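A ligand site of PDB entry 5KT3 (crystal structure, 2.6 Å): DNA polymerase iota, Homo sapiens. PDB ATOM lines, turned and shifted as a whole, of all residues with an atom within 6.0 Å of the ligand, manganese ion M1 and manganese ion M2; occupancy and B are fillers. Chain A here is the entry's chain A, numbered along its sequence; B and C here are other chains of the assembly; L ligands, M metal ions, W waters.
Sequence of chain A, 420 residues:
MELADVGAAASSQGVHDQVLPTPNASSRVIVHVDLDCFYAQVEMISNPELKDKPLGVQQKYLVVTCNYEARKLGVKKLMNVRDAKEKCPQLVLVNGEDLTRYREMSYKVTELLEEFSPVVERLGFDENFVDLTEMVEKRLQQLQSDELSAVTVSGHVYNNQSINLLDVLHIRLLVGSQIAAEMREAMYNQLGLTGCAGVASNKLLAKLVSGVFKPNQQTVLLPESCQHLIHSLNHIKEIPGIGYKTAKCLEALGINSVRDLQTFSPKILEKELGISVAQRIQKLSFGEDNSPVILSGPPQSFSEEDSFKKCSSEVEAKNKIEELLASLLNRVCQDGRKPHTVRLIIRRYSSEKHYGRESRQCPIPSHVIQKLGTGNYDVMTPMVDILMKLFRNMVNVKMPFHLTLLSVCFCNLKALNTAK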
ATOM      1  N   ASP A  34      13.986  13.915  21.393  1.00  0.00           N
ATOM      2  CA  ASP A  34      15.288  14.332  21.901  1.00  0.00           C
ATOM      3  C   ASP A  34      15.525  15.755  21.453  1.00  0.00           C
ATOM      4  O   ASP A  34      15.279  16.090  20.291  1.00  0.00           O
ATOM      5  CB  ASP A  34      16.422  13.429  21.379  1.00  0.00           C
ATOM      6  CG  ASP A  34      17.783  13.856  21.877  1.00  0.00           C
ATOM      7  OD1 ASP A  34      18.510  13.005  22.392  1.00  0.00           O
ATOM      8  OD2 ASP A  34      18.154  15.046  21.728  1.00  0.00           O
ATOM      9  N   LEU A  35      16.055  16.595  22.343  1.00  0.00           N
ATOM     10  CA  LEU A  35      16.132  18.004  22.028  1.00  0.00           C
ATOM     11  C   LEU A  35      17.438  18.348  21.319  1.00  0.00           C
ATOM     12  O   LEU A  35      18.479  17.738  21.578  1.00  0.00           O
ATOM     13  CB  LEU A  35      16.000  18.834  23.295  1.00  0.00           C
ATOM     14  CG  LEU A  35      14.620  18.671  23.913  1.00  0.00           C
ATOM     15  CD1 LEU A  35      14.530  19.468  25.179  1.00  0.00           C
ATOM     16  CD2 LEU A  35      13.593  19.167  22.947  1.00  0.00           C
ATOM     17  N   ASP A  36      17.366  19.315  20.414  1.00  0.00           N
ATOM     18  CA  ASP A  36      18.544  19.808  19.713  1.00  0.00           C
ATOM     19  C   ASP A  36      19.458  20.576  20.666  1.00  0.00           C
ATOM     20  O   ASP A  36      19.019  21.548  21.305  1.00  0.00           O
ATOM     21  CB  ASP A  36      18.145  20.725  18.564  1.00  0.00           C
ATOM     22  CG  ASP A  36      17.187  20.080  17.583  1.00  0.00           C
ATOM     23  OD1 ASP A  36      17.259  18.848  17.377  1.00  0.00           O
ATOM     24  OD2 ASP A  36      16.376  20.823  17.014  1.00  0.00           O
ATOM     25  N   CYS A  37      20.734  20.170  20.716  1.00  0.00           N
ATOM     26  CA  CYS A  37      21.785  20.820  21.508  1.00  0.00           C
ATOM     27  C   CYS A  37      21.240  21.476  22.765  1.00  0.00           C
ATOM     28  O   CYS A  37      21.422  22.688  22.983  1.00  0.00           O
ATOM     29  CB  CYS A  37      22.555  21.825  20.646  1.00  0.00           C
ATOM     30  SG  CYS A  37      21.523  23.092  19.841  1.00  0.00           S
ATOM     31  N   PHE A  38      20.581  20.675  23.608  1.00  0.00           N
ATOM     32  CA  PHE A  38      19.648  21.184  24.610  1.00  0.00           C
ATOM     33  C   PHE A  38      20.213  22.372  25.372  1.00  0.00           C
ATOM     34  O   PHE A  38      19.635  23.473  25.347  1.00  0.00           O
ATOM     35  CB  PHE A  38      19.265  20.046  25.575  1.00  0.00           C
ATOM     36  CG  PHE A  38      18.301  20.457  26.638  1.00  0.00           C
ATOM     37  CD1 PHE A  38      17.210  21.268  26.339  1.00  0.00           C
ATOM     38  CD2 PHE A  38      18.485  20.044  27.942  1.00  0.00           C
ATOM     39  CE1 PHE A  38      16.311  21.657  27.335  1.00  0.00           C
ATOM     40  CE2 PHE A  38      17.600  20.421  28.949  1.00  0.00           C
ATOM     41  CZ  PHE A  38      16.507  21.237  28.643  1.00  0.00           C
ATOM     42  N   TYR A  39      21.317  22.168  26.093  1.00  0.00           N
ATOM     43  CA  TYR A  39      21.830  23.247  26.953  1.00  0.00           C
ATOM     44  C   TYR A  39      22.108  24.487  26.110  1.00  0.00           C
ATOM     45  O   TYR A  39      21.647  25.599  26.428  1.00  0.00           O
ATOM     46  CB  TYR A  39      23.109  22.812  27.675  1.00  0.00           C
ATOM     47  CG  TYR A  39      22.932  21.825  28.805  1.00  0.00           C
ATOM     48  CD1 TYR A  39      21.693  21.242  29.089  1.00  0.00           C
ATOM     49  CD2 TYR A  39      24.023  21.477  29.608  1.00  0.00           C
ATOM     50  CE1 TYR A  39      21.552  20.322  30.130  1.00  0.00           C
ATOM     51  CE2 TYR A  39      23.894  20.587  30.658  1.00  0.00           C
ATOM     52  CZ  TYR A  39      22.668  20.009  30.916  1.00  0.00           C
ATOM     53  OH  TYR A  39      22.554  19.119  31.947  1.00  0.00           O
ATOM     54  N   ALA A  40      22.858  24.310  25.020  1.00  0.00           N
ATOM     55  CA  ALA A  40      23.121  25.395  24.100  1.00  0.00           C
ATOM     56  C   ALA A  40      21.827  26.054  23.649  1.00  0.00           C
ATOM     57  O   ALA A  40      21.750  27.280  23.577  1.00  0.00           O
ATOM     58  CB  ALA A  40      23.917  24.886  22.907  1.00  0.00           C
ATOM     59  N   GLN A  59      31.438  23.050  31.316  1.00  0.00           N
ATOM     60  CA  GLN A  59      31.347  22.663  32.715  1.00  0.00           C
ATOM     61  C   GLN A  59      32.749  22.241  33.137  1.00  0.00           C
ATOM     62  O   GLN A  59      33.229  21.175  32.744  1.00  0.00           O
ATOM     63  CB  GLN A  59      30.340  21.525  32.903  1.00  0.00           C
ATOM     64  CG  GLN A  59      28.900  21.878  32.558  1.00  0.00           C
ATOM     65  CD  GLN A  59      27.948  20.719  32.791  1.00  0.00           C
ATOM     66  OE1 GLN A  59      28.318  19.560  32.584  1.00  0.00           O
ATOM     67  NE2 GLN A  59      26.737  21.016  33.255  1.00  0.00           N
ATOM     68  N   VAL A  64      30.286  20.513  27.094  1.00  0.00           N
ATOM     69  CA  VAL A  64      29.415  19.361  27.283  1.00  0.00           C
ATOM     70  C   VAL A  64      28.456  19.243  26.108  1.00  0.00           C
ATOM     71  O   VAL A  64      28.093  18.127  25.703  1.00  0.00           O
ATOM     72  CB  VAL A  64      28.740  19.465  28.668  1.00  0.00           C
ATOM     73  CG1 VAL A  64      27.542  20.412  28.674  1.00  0.00           C
ATOM     74  CG2 VAL A  64      28.371  18.088  29.172  1.00  0.00           C
ATOM     75  N   THR A  65      28.103  20.363  25.481  1.00  0.00           N
ATOM     76  CA  THR A  65      27.439  20.352  24.186  1.00  0.00           C
ATOM     77  C   THR A  65      27.814  21.650  23.474  1.00  0.00           C
ATOM     78  O   THR A  65      28.400  22.564  24.056  1.00  0.00           O
ATOM     79  CB  THR A  65      25.925  20.190  24.326  1.00  0.00           C
ATOM     80  OG1 THR A  65      25.314  20.082  23.025  1.00  0.00           O
ATOM     81  CG2 THR A  65      25.318  21.365  25.061  1.00  0.00           C
ATOM     82  N   CYS A  66      27.460  21.707  22.183  1.00  0.00           N
ATOM     83  CA  CYS A  66      27.643  22.925  21.406  1.00  0.00           C
ATOM     84  C   CYS A  66      26.520  23.006  20.378  1.00  0.00           C
ATOM     85  O   CYS A  66      25.912  21.988  20.039  1.00  0.00           O
ATOM     86  CB  CYS A  66      28.992  22.945  20.699  1.00  0.00           C
ATOM     87  SG  CYS A  66      29.211  21.519  19.659  1.00  0.00           S
ATOM     88  N   TYR A  68      24.795  24.037  16.553  1.00  0.00           N
ATOM     89  CA  TYR A  68      25.122  23.383  15.297  1.00  0.00           C
ATOM     90  C   TYR A  68      26.100  24.194  14.446  1.00  0.00           C
ATOM     91  O   TYR A  68      26.849  23.592  13.666  1.00  0.00           O
ATOM     92  CB  TYR A  68      23.834  23.042  14.551  1.00  0.00           C
ATOM     93  CG  TYR A  68      23.278  21.733  15.063  1.00  0.00           C
ATOM     94  CD1 TYR A  68      22.582  21.667  16.278  1.00  0.00           C
ATOM     95  CD2 TYR A  68      23.494  20.539  14.379  1.00  0.00           C
ATOM     96  CE1 TYR A  68      22.090  20.453  16.772  1.00  0.00           C
ATOM     97  CE2 TYR A  68      23.001  19.317  14.867  1.00  0.00           C
ATOM     98  CZ  TYR A  68      22.298  19.284  16.059  1.00  0.00           C
ATOM     99  OH  TYR A  68      21.828  18.086  16.560  1.00  0.00           O
ATOM    100  N   ARG A  71      29.270  22.810  15.560  1.00  0.00           N
ATOM    101  CA  ARG A  71      29.532  21.486  15.022  1.00  0.00           C
ATOM    102  C   ARG A  71      29.972  21.555  13.561  1.00  0.00           C
ATOM    103  O   ARG A  71      30.763  20.717  13.121  1.00  0.00           O
ATOM    104  CB  ARG A  71      28.297  20.595  15.170  1.00  0.00           C
ATOM    105  CG  ARG A  71      28.009  20.214  16.610  1.00  0.00           C
ATOM    106  CD  ARG A  71      26.712  19.441  16.772  1.00  0.00           C
ATOM    107  NE  ARG A  71      26.094  19.747  18.058  1.00  0.00           N
ATOM    108  CZ  ARG A  71      25.249  18.950  18.716  1.00  0.00           C
ATOM    109  NH1 ARG A  71      24.919  17.760  18.235  1.00  0.00           N
ATOM    110  NH2 ARG A  71      24.746  19.359  19.866  1.00  0.00           N
ATOM    111  N   LYS A  77      30.418  17.103  20.782  1.00  0.00           N
ATOM    112  CA  LYS A  77      29.919  17.002  22.137  1.00  0.00           C
ATOM    113  C   LYS A  77      30.934  16.294  23.030  1.00  0.00           C
ATOM    114  O   LYS A  77      31.561  15.320  22.617  1.00  0.00           O
ATOM    115  CB  LYS A  77      28.582  16.259  22.161  1.00  0.00           C
ATOM    116  CG  LYS A  77      27.463  17.015  21.425  1.00  0.00           C
ATOM    117  CD  LYS A  77      26.192  16.177  21.262  1.00  0.00           C
ATOM    118  CE  LYS A  77      26.424  14.946  20.445  1.00  0.00           C
ATOM    119  NZ  LYS A  77      25.197  14.577  19.654  1.00  0.00           N
ATOM    120  N   LEU A  78      31.092  16.803  24.252  1.00  0.00           N
ATOM    121  CA  LEU A  78      31.979  16.231  25.264  1.00  0.00           C
ATOM    122  C   LEU A  78      33.442  16.322  24.858  1.00  0.00           C
ATOM    123  O   LEU A  78      34.243  15.448  25.191  1.00  0.00           O
ATOM    124  CB  LEU A  78      31.572  14.790  25.585  1.00  0.00           C
ATOM    125  CG  LEU A  78      30.095  14.619  25.966  1.00  0.00           C
ATOM    126  CD1 LEU A  78      29.703  13.153  26.041  1.00  0.00           C
ATOM    127  CD2 LEU A  78      29.782  15.341  27.278  1.00  0.00           C
ATOM    128  N   LEU A 123      14.055  10.369  30.053  1.00  0.00           N
ATOM    129  CA  LEU A 123      15.376   9.763  30.050  1.00  0.00           C
ATOM    130  C   LEU A 123      16.386  10.899  30.023  1.00  0.00           C
ATOM    131  O   LEU A 123      16.511  11.592  29.006  1.00  0.00           O
ATOM    132  CB  LEU A 123      15.567   8.815  28.865  1.00  0.00           C
ATOM    133  CG  LEU A 123      16.877   8.018  28.874  1.00  0.00           C
ATOM    134  CD1 LEU A 123      17.018   7.152  30.148  1.00  0.00           C
ATOM    135  CD2 LEU A 123      16.999   7.180  27.603  1.00  0.00           C
ATOM    136  N   PHE A 125      17.683  14.690  30.853  1.00  0.00           N
ATOM    137  CA  PHE A 125      16.953  15.949  30.864  1.00  0.00           C
ATOM    138  C   PHE A 125      16.262  16.269  29.554  1.00  0.00           C
ATOM    139  O   PHE A 125      15.387  17.134  29.551  1.00  0.00           O
ATOM    140  CB  PHE A 125      17.881  17.133  31.179  1.00  0.00           C
ATOM    141  CG  PHE A 125      18.158  17.332  32.639  1.00  0.00           C
ATOM    142  CD1 PHE A 125      18.768  18.514  33.080  1.00  0.00           C
ATOM    143  CD2 PHE A 125      17.832  16.358  33.566  1.00  0.00           C
ATOM    144  CE1 PHE A 125      19.044  18.705  34.422  1.00  0.00           C
ATOM    145  CE2 PHE A 125      18.100  16.556  34.918  1.00  0.00           C
ATOM    146  CZ  PHE A 125      18.716  17.723  35.344  1.00  0.00           C
ATOM    147  N   ASP A 126      16.657  15.657  28.438  1.00  0.00           N
ATOM    148  CA  ASP A 126      16.202  16.169  27.142  1.00  0.00           C
ATOM    149  C   ASP A 126      15.521  15.123  26.281  1.00  0.00           C
ATOM    150  O   ASP A 126      15.292  15.386  25.092  1.00  0.00           O
ATOM    151  CB  ASP A 126      17.369  16.814  26.386  1.00  0.00           C
ATOM    152  CG  ASP A 126      18.124  15.835  25.504  1.00  0.00           C
ATOM    153  OD1 ASP A 126      18.321  14.678  25.942  1.00  0.00           O
ATOM    154  OD2 ASP A 126      18.509  16.208  24.370  1.00  0.00           O
ATOM    155  N   GLU A 127      15.147  13.970  26.833  1.00  0.00           N
ATOM    156  CA  GLU A 127      14.506  12.912  26.073  1.00  0.00           C
ATOM    157  C   GLU A 127      13.244  12.450  26.773  1.00  0.00           C
ATOM    158  O   GLU A 127      13.209  12.324  28.002  1.00  0.00           O
ATOM    159  CB  GLU A 127      15.437  11.715  25.862  1.00  0.00           C
ATOM    160  CG  GLU A 127      16.540  12.005  24.867  1.00  0.00           C
ATOM    161  CD  GLU A 127      17.586  10.912  24.821  1.00  0.00           C
ATOM    162  OE1 GLU A 127      17.218   9.710  24.793  1.00  0.00           O
ATOM    163  OE2 GLU A 127      18.787  11.272  24.817  1.00  0.00           O
ATOM    164  N   LYS A 207      13.954   5.226  19.790  1.00  0.00           N
ATOM    165  CA  LYS A 207      15.123   6.010  20.170  1.00  0.00           C
ATOM    166  C   LYS A 207      16.238   5.914  19.132  1.00  0.00           C
ATOM    167  O   LYS A 207      16.978   6.887  18.937  1.00  0.00           O
ATOM    168  CB  LYS A 207      15.648   5.592  21.541  1.00  0.00           C
ATOM    169  CG  LYS A 207      16.835   6.427  22.030  1.00  0.00           C
ATOM    170  CD  LYS A 207      17.468   5.815  23.278  1.00  0.00           C
ATOM    171  CE  LYS A 207      18.122   6.854  24.154  1.00  0.00           C
ATOM    172  NZ  LYS A 207      19.230   7.537  23.491  1.00  0.00           N
ATOM    173  N   LYS A 214      18.885  14.822  11.751  1.00  0.00           N
ATOM    174  CA  LYS A 214      19.107  15.870  12.716  1.00  0.00           C
ATOM    175  C   LYS A 214      19.635  17.121  12.025  1.00  0.00           C
ATOM    176  O   LYS A 214      20.350  17.020  11.040  1.00  0.00           O
ATOM    177  CB  LYS A 214      20.133  15.429  13.759  1.00  0.00           C
ATOM    178  CG  LYS A 214      19.683  14.309  14.638  1.00  0.00           C
ATOM    179  CD  LYS A 214      20.889  13.712  15.336  1.00  0.00           C
ATOM    180  CE  LYS A 214      21.452  14.649  16.356  1.00  0.00           C
ATOM    181  NZ  LYS A 214      22.657  14.038  16.974  1.00  0.00           N
ATOM    182  N   PRO A 215      19.333  18.302  12.586  1.00  0.00           N
ATOM    183  CA  PRO A 215      18.448  18.448  13.747  1.00  0.00           C
ATOM    184  C   PRO A 215      17.029  18.823  13.371  1.00  0.00           C
ATOM    185  O   PRO A 215      16.741  18.990  12.184  1.00  0.00           O
ATOM    186  CB  PRO A 215      19.114  19.573  14.531  1.00  0.00           C
ATOM    187  CG  PRO A 215      19.698  20.439  13.467  1.00  0.00           C
ATOM    188  CD  PRO A 215      20.125  19.509  12.348  1.00  0.00           C
ATOM    189  P    DC B   7      22.038   7.326  26.097  1.00  0.00           P
ATOM    190  OP1  DC B   7      21.329   7.412  24.805  1.00  0.00           O
ATOM    191  OP2  DC B   7      23.466   6.919  26.208  1.00  0.00           O
ATOM    192  O5'  DC B   7      21.855   8.761  26.750  1.00  0.00           O
ATOM    193  C5'  DC B   7      20.646   9.450  26.531  1.00  0.00           C
ATOM    194  C4'  DC B   7      20.676  10.787  27.222  1.00  0.00           C
ATOM    195  O4'  DC B   7      20.998  10.586  28.602  1.00  0.00           O
ATOM    196  C3'  DC B   7      21.750  11.729  26.731  1.00  0.00           C
ATOM    197  O3'  DC B   7      21.296  12.415  25.574  1.00  0.00           O
ATOM    198  C2'  DC B   7      21.869  12.674  27.911  1.00  0.00           C
ATOM    199  C1'  DC B   7      21.616  11.751  29.108  1.00  0.00           C
ATOM    200  N1   DC B   7      22.861  11.368  29.791  1.00  0.00           N
ATOM    201  C2   DC B   7      23.434  12.269  30.694  1.00  0.00           C
ATOM    202  O2   DC B   7      22.881  13.345  30.900  1.00  0.00           O
ATOM    203  N3   DC B   7      24.578  11.918  31.313  1.00  0.00           N
ATOM    204  C4   DC B   7      25.143  10.746  31.061  1.00  0.00           C
ATOM    205  N4   DC B   7      26.270  10.445  31.703  1.00  0.00           N
ATOM    206  C5   DC B   7      24.577   9.817  30.144  1.00  0.00           C
ATOM    207  C6   DC B   7      23.447  10.169  29.535  1.00  0.00           C
ATOM    208  P    DG C   3      36.174  17.821  34.683  1.00  0.00           P
ATOM    209  OP1  DG C   3      36.447  18.682  33.508  1.00  0.00           O
ATOM    210  OP2  DG C   3      36.976  17.964  35.928  1.00  0.00           O
ATOM    211  O5'  DG C   3      34.668  17.952  35.148  1.00  0.00           O
ATOM    212  C5'  DG C   3      33.623  17.622  34.267  1.00  0.00           C
ATOM    213  C4'  DG C   3      32.476  18.574  34.493  1.00  0.00           C
ATOM    214  O4'  DG C   3      31.409  18.316  33.545  1.00  0.00           O
ATOM    215  C3'  DG C   3      31.834  18.479  35.858  1.00  0.00           C
ATOM    216  O3'  DG C   3      31.254  19.731  36.144  1.00  0.00           O
ATOM    217  C2'  DG C   3      30.771  17.393  35.630  1.00  0.00           C
ATOM    218  C1'  DG C   3      30.299  17.733  34.214  1.00  0.00           C
ATOM    219  N9   DG C   3      29.870  16.597  33.387  1.00  0.00           N
ATOM    220  C8   DG C   3      28.785  16.574  32.556  1.00  0.00           C
ATOM    221  N7   DG C   3      28.652  15.468  31.896  1.00  0.00           N
ATOM    222  C5   DG C   3      29.733  14.694  32.312  1.00  0.00           C
ATOM    223  C6   DG C   3      30.111  13.389  31.932  1.00  0.00           C
ATOM    224  O6   DG C   3      29.539  12.630  31.126  1.00  0.00           O
ATOM    225  N1   DG C   3      31.264  12.976  32.576  1.00  0.00           N
ATOM    226  C2   DG C   3      31.968  13.743  33.484  1.00  0.00           C
ATOM    227  N2   DG C   3      33.062  13.176  34.011  1.00  0.00           N
ATOM    228  N3   DG C   3      31.621  14.971  33.855  1.00  0.00           N
ATOM    229  C4   DG C   3      30.494  15.379  33.226  1.00  0.00           C
ATOM    230  P    DG C   4      30.783  20.073  37.622  1.00  0.00           P
ATOM    231  OP1  DG C   4      30.896  21.526  37.882  1.00  0.00           O
ATOM    232  OP2  DG C   4      31.443  19.079  38.469  1.00  0.00           O
ATOM    233  O5'  DG C   4      29.227  19.725  37.584  1.00  0.00           O
ATOM    234  C5'  DG C   4      28.357  20.461  36.766  1.00  0.00           C
ATOM    235  C4'  DG C   4      27.044  19.749  36.699  1.00  0.00           C
ATOM    236  O4'  DG C   4      27.199  18.554  35.870  1.00  0.00           O
ATOM    237  C3'  DG C   4      26.550  19.229  38.053  1.00  0.00           C
ATOM    238  O3'  DG C   4      25.172  19.552  38.223  1.00  0.00           O
ATOM    239  C2'  DG C   4      26.776  17.722  37.954  1.00  0.00           C
ATOM    240  C1'  DG C   4      26.504  17.522  36.478  1.00  0.00           C
ATOM    241  N9   DG C   4      26.969  16.255  35.968  1.00  0.00           N
ATOM    242  C8   DG C   4      28.036  15.524  36.414  1.00  0.00           C
ATOM    243  N7   DG C   4      28.199  14.401  35.768  1.00  0.00           N
ATOM    244  C5   DG C   4      27.153  14.374  34.853  1.00  0.00           C
ATOM    245  C6   DG C   4      26.813  13.404  33.884  1.00  0.00           C
ATOM    246  O6   DG C   4      27.384  12.339  33.628  1.00  0.00           O
ATOM    247  N1   DG C   4      25.679  13.790  33.155  1.00  0.00           N
ATOM    248  C2   DG C   4      24.984  14.943  33.349  1.00  0.00           C
ATOM    249  N2   DG C   4      23.916  15.137  32.568  1.00  0.00           N
ATOM    250  N3   DG C   4      25.289  15.850  34.260  1.00  0.00           N
ATOM    251  C4   DG C   4      26.384  15.502  34.967  1.00  0.00           C
HETATM  252  P1  LIG L   1      21.804  16.677  20.174  1.00  0.00           P
HETATM  253  O1  LIG L   1      20.806  15.838  20.952  1.00  0.00           O
HETATM  254  O2  LIG L   1      22.848  15.840  19.451  1.00  0.00           O
HETATM  255  O3  LIG L   1      21.177  17.767  19.346  1.00  0.00           O
HETATM  256  P2  LIG L   1      22.364  17.534  22.838  1.00  0.00           P
HETATM  257  O4  LIG L   1      23.105  18.697  23.413  1.00  0.00           O
HETATM  258  O5  LIG L   1      20.885  17.497  23.119  1.00  0.00           O
HETATM  259  O6  LIG L   1      22.603  17.575  21.251  1.00  0.00           O
HETATM  260  P3  LIG L   1      22.283  14.975  24.249  1.00  0.00           P
HETATM  261  O7  LIG L   1      23.119  13.717  24.357  1.00  0.00           O
HETATM  262  O8  LIG L   1      20.940  14.915  23.604  1.00  0.00           O
HETATM  263  N1  LIG L   1      23.248  16.124  23.358  1.00  0.00           N
HETATM  264  O9  LIG L   1      22.176  15.499  25.787  1.00  0.00           O
HETATM  265  C1  LIG L   1      21.291  16.527  26.177  1.00  0.00           C
HETATM  266  C2  LIG L   1      21.983  17.536  27.112  1.00  0.00           C
HETATM  267  O10 LIG L   1      22.422  16.887  28.292  1.00  0.00           O
HETATM  268  C3  LIG L   1      23.226  18.190  26.518  1.00  0.00           C
HETATM  269  O11 LIG L   1      22.914  19.407  25.827  1.00  0.00           O
HETATM  270  C4  LIG L   1      24.112  18.441  27.708  1.00  0.00           C
HETATM  271  C5  LIG L   1      23.669  17.410  28.732  1.00  0.00           C
HETATM  272  N2  LIG L   1      24.596  16.276  28.810  1.00  0.00           N
HETATM  273  C6  LIG L   1      25.598  16.298  29.790  1.00  0.00           C
HETATM  274  N3  LIG L   1      26.466  15.269  29.897  1.00  0.00           N
HETATM  275  C7  LIG L   1      26.361  14.203  29.085  1.00  0.00           C
HETATM  276  C8  LIG L   1      25.372  14.161  28.111  1.00  0.00           C
HETATM  277  C9  LIG L   1      24.481  15.223  28.000  1.00  0.00           C
HETATM  278  O12 LIG L   1      25.695  17.268  30.561  1.00  0.00           O
HETATM  279  N4  LIG L   1      27.253  13.186  29.237  1.00  0.00           N
HETATM  280 MN    MN M   1      19.534  16.192  22.541  1.00  0.00          MN
HETATM  281 MN    MN M   2      19.647  13.260  24.329  1.00  0.00          MN
HETATM  282  O   HOH W   1      27.153  10.679  27.549  1.00  0.00           O
HETATM  283  O   HOH W   2      24.926  18.031  32.887  1.00  0.00           O
HETATM  284  O   HOH W   3      25.790  13.629  24.345  1.00  0.00           O
HETATM  285  O   HOH W   4      21.676  12.995  21.006  1.00  0.00           O
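The side-chain carboxylate (OE1) of Glu 127 is in salt-bridge range of the side-chain amino group (NZ) of Lys 207 (3.2 Å). N2 of DG 4 of chain C sits close to O2 of DC 7 of chain B, at 2.7 Å. OP1 of DC 7 of chain B is in salt-bridge range of NZ of Lys 207, 2.5 Å away. The side-chain hydroxyl (OG1) of Thr 65 lies within hydrogen-bond range of the guanidinium group (NH2) of Arg 71 (3.3 Å). N9 of DG 3 of chain C lies close to OE1 of Gln 59. The backbone carbonyl oxygen (O) of Cys 66 is in hydrogen-bond range of the guanidinium group (NH2) of Arg 71, at 2.9 Å.
Three residues have an atom within 4 Å of manganese ion M1: Asp 34, Leu 35 and Asp 126. Along chain A the residues within 4 Å of manganese ion M1 span positions 34 to 126.
Within 4 Å of manganese ion M2: Asp 34, Asp 126, Glu 127 and DC 7 of chain B.
Water W2 lies within hydrogen-bond range of an oxygen (O12) of the ligand (2.6 Å), N3 of DG 4 of chain C (2.6 Å) and the side-chain hydroxyl (OH) of Tyr 39 (2.8 Å).
An oxygen (O4) of the ligand sits at hydrogen-bond distance from the side-chain hydroxyl of Thr 65, 2.6 Å away. The side-chain amino group of Lys 77 lies within salt-bridge range of an oxygen (O2) of the ligand. O3 of the ligand is in hydrogen-bond range of N of Cys 37 (2.8 Å). The side-chain hydroxyl of Tyr 68 lies within hydrogen-bond range of an oxygen (O3) of the ligand, 2.9 Å away. O6 of DG 3 of chain C sits at hydrogen-bond distance from N4 of the ligand, at 3.0 Å. The side-chain amino group of Lys 214 is in salt-bridge range of an oxygen (O2) of the ligand (3.1 Å). NH1 of Arg 71 lies within salt-bridge range of O2 of the ligand (3.1 Å). The backbone NH of Tyr 39 lies within hydrogen-bond range of an oxygen (O11) of the ligand (3.2 Å). N of Phe 38 is in hydrogen-bond range of O4 of the ligand (3.2 Å).
O12 of the ligand lies close to N2 of DG 4 of chain C. Merely in contact with the ligand: Val 64 (3.1 Å), Asp 36 (3.4 Å) and Leu 78 (3.9 Å). Hydrophobic or aromatic side chains within 4 Å of the ligand: Phe 38, Tyr 39, Val 64, Tyr 68 and Leu 78. 17 residues have an atom within 4 Å of the ligand: Asp 34, Leu 35, Asp 36, Cys 37, Phe 38, Tyr 39, Val 64, Thr 65, Tyr 68, Arg 71, Lys 77, Leu 78, Asp 126, Lys 214, DC 7 of chain B, DG 3 of chain C and DG 4 of chain C. The nearest printed residue that does not touch the ligand is Gln 59 (4.03 Å).
Manganese ion M1 is bound by O5 of the ligand (2.0 Å), OD2 of Asp 34 (2.0 Å), O1 of the ligand (2.1 Å), OD2 of Asp 126 (2.1 Å), O of Leu 35 (2.1 Å) and O8 of the ligand (2.2 Å). Manganese ion M1 has six donor atoms within binding distance.
Manganese ion M2 is bound by the side-chain carboxylate (OE2) of Glu 127, an oxygen (O8) of the ligand, O3' of DC 7 of chain B, the side-chain carboxylate (OD1) of Asp 34 and the side-chain carboxylate (OD1) of Asp 126. Manganese ion M2 has five donor atoms within binding distance.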
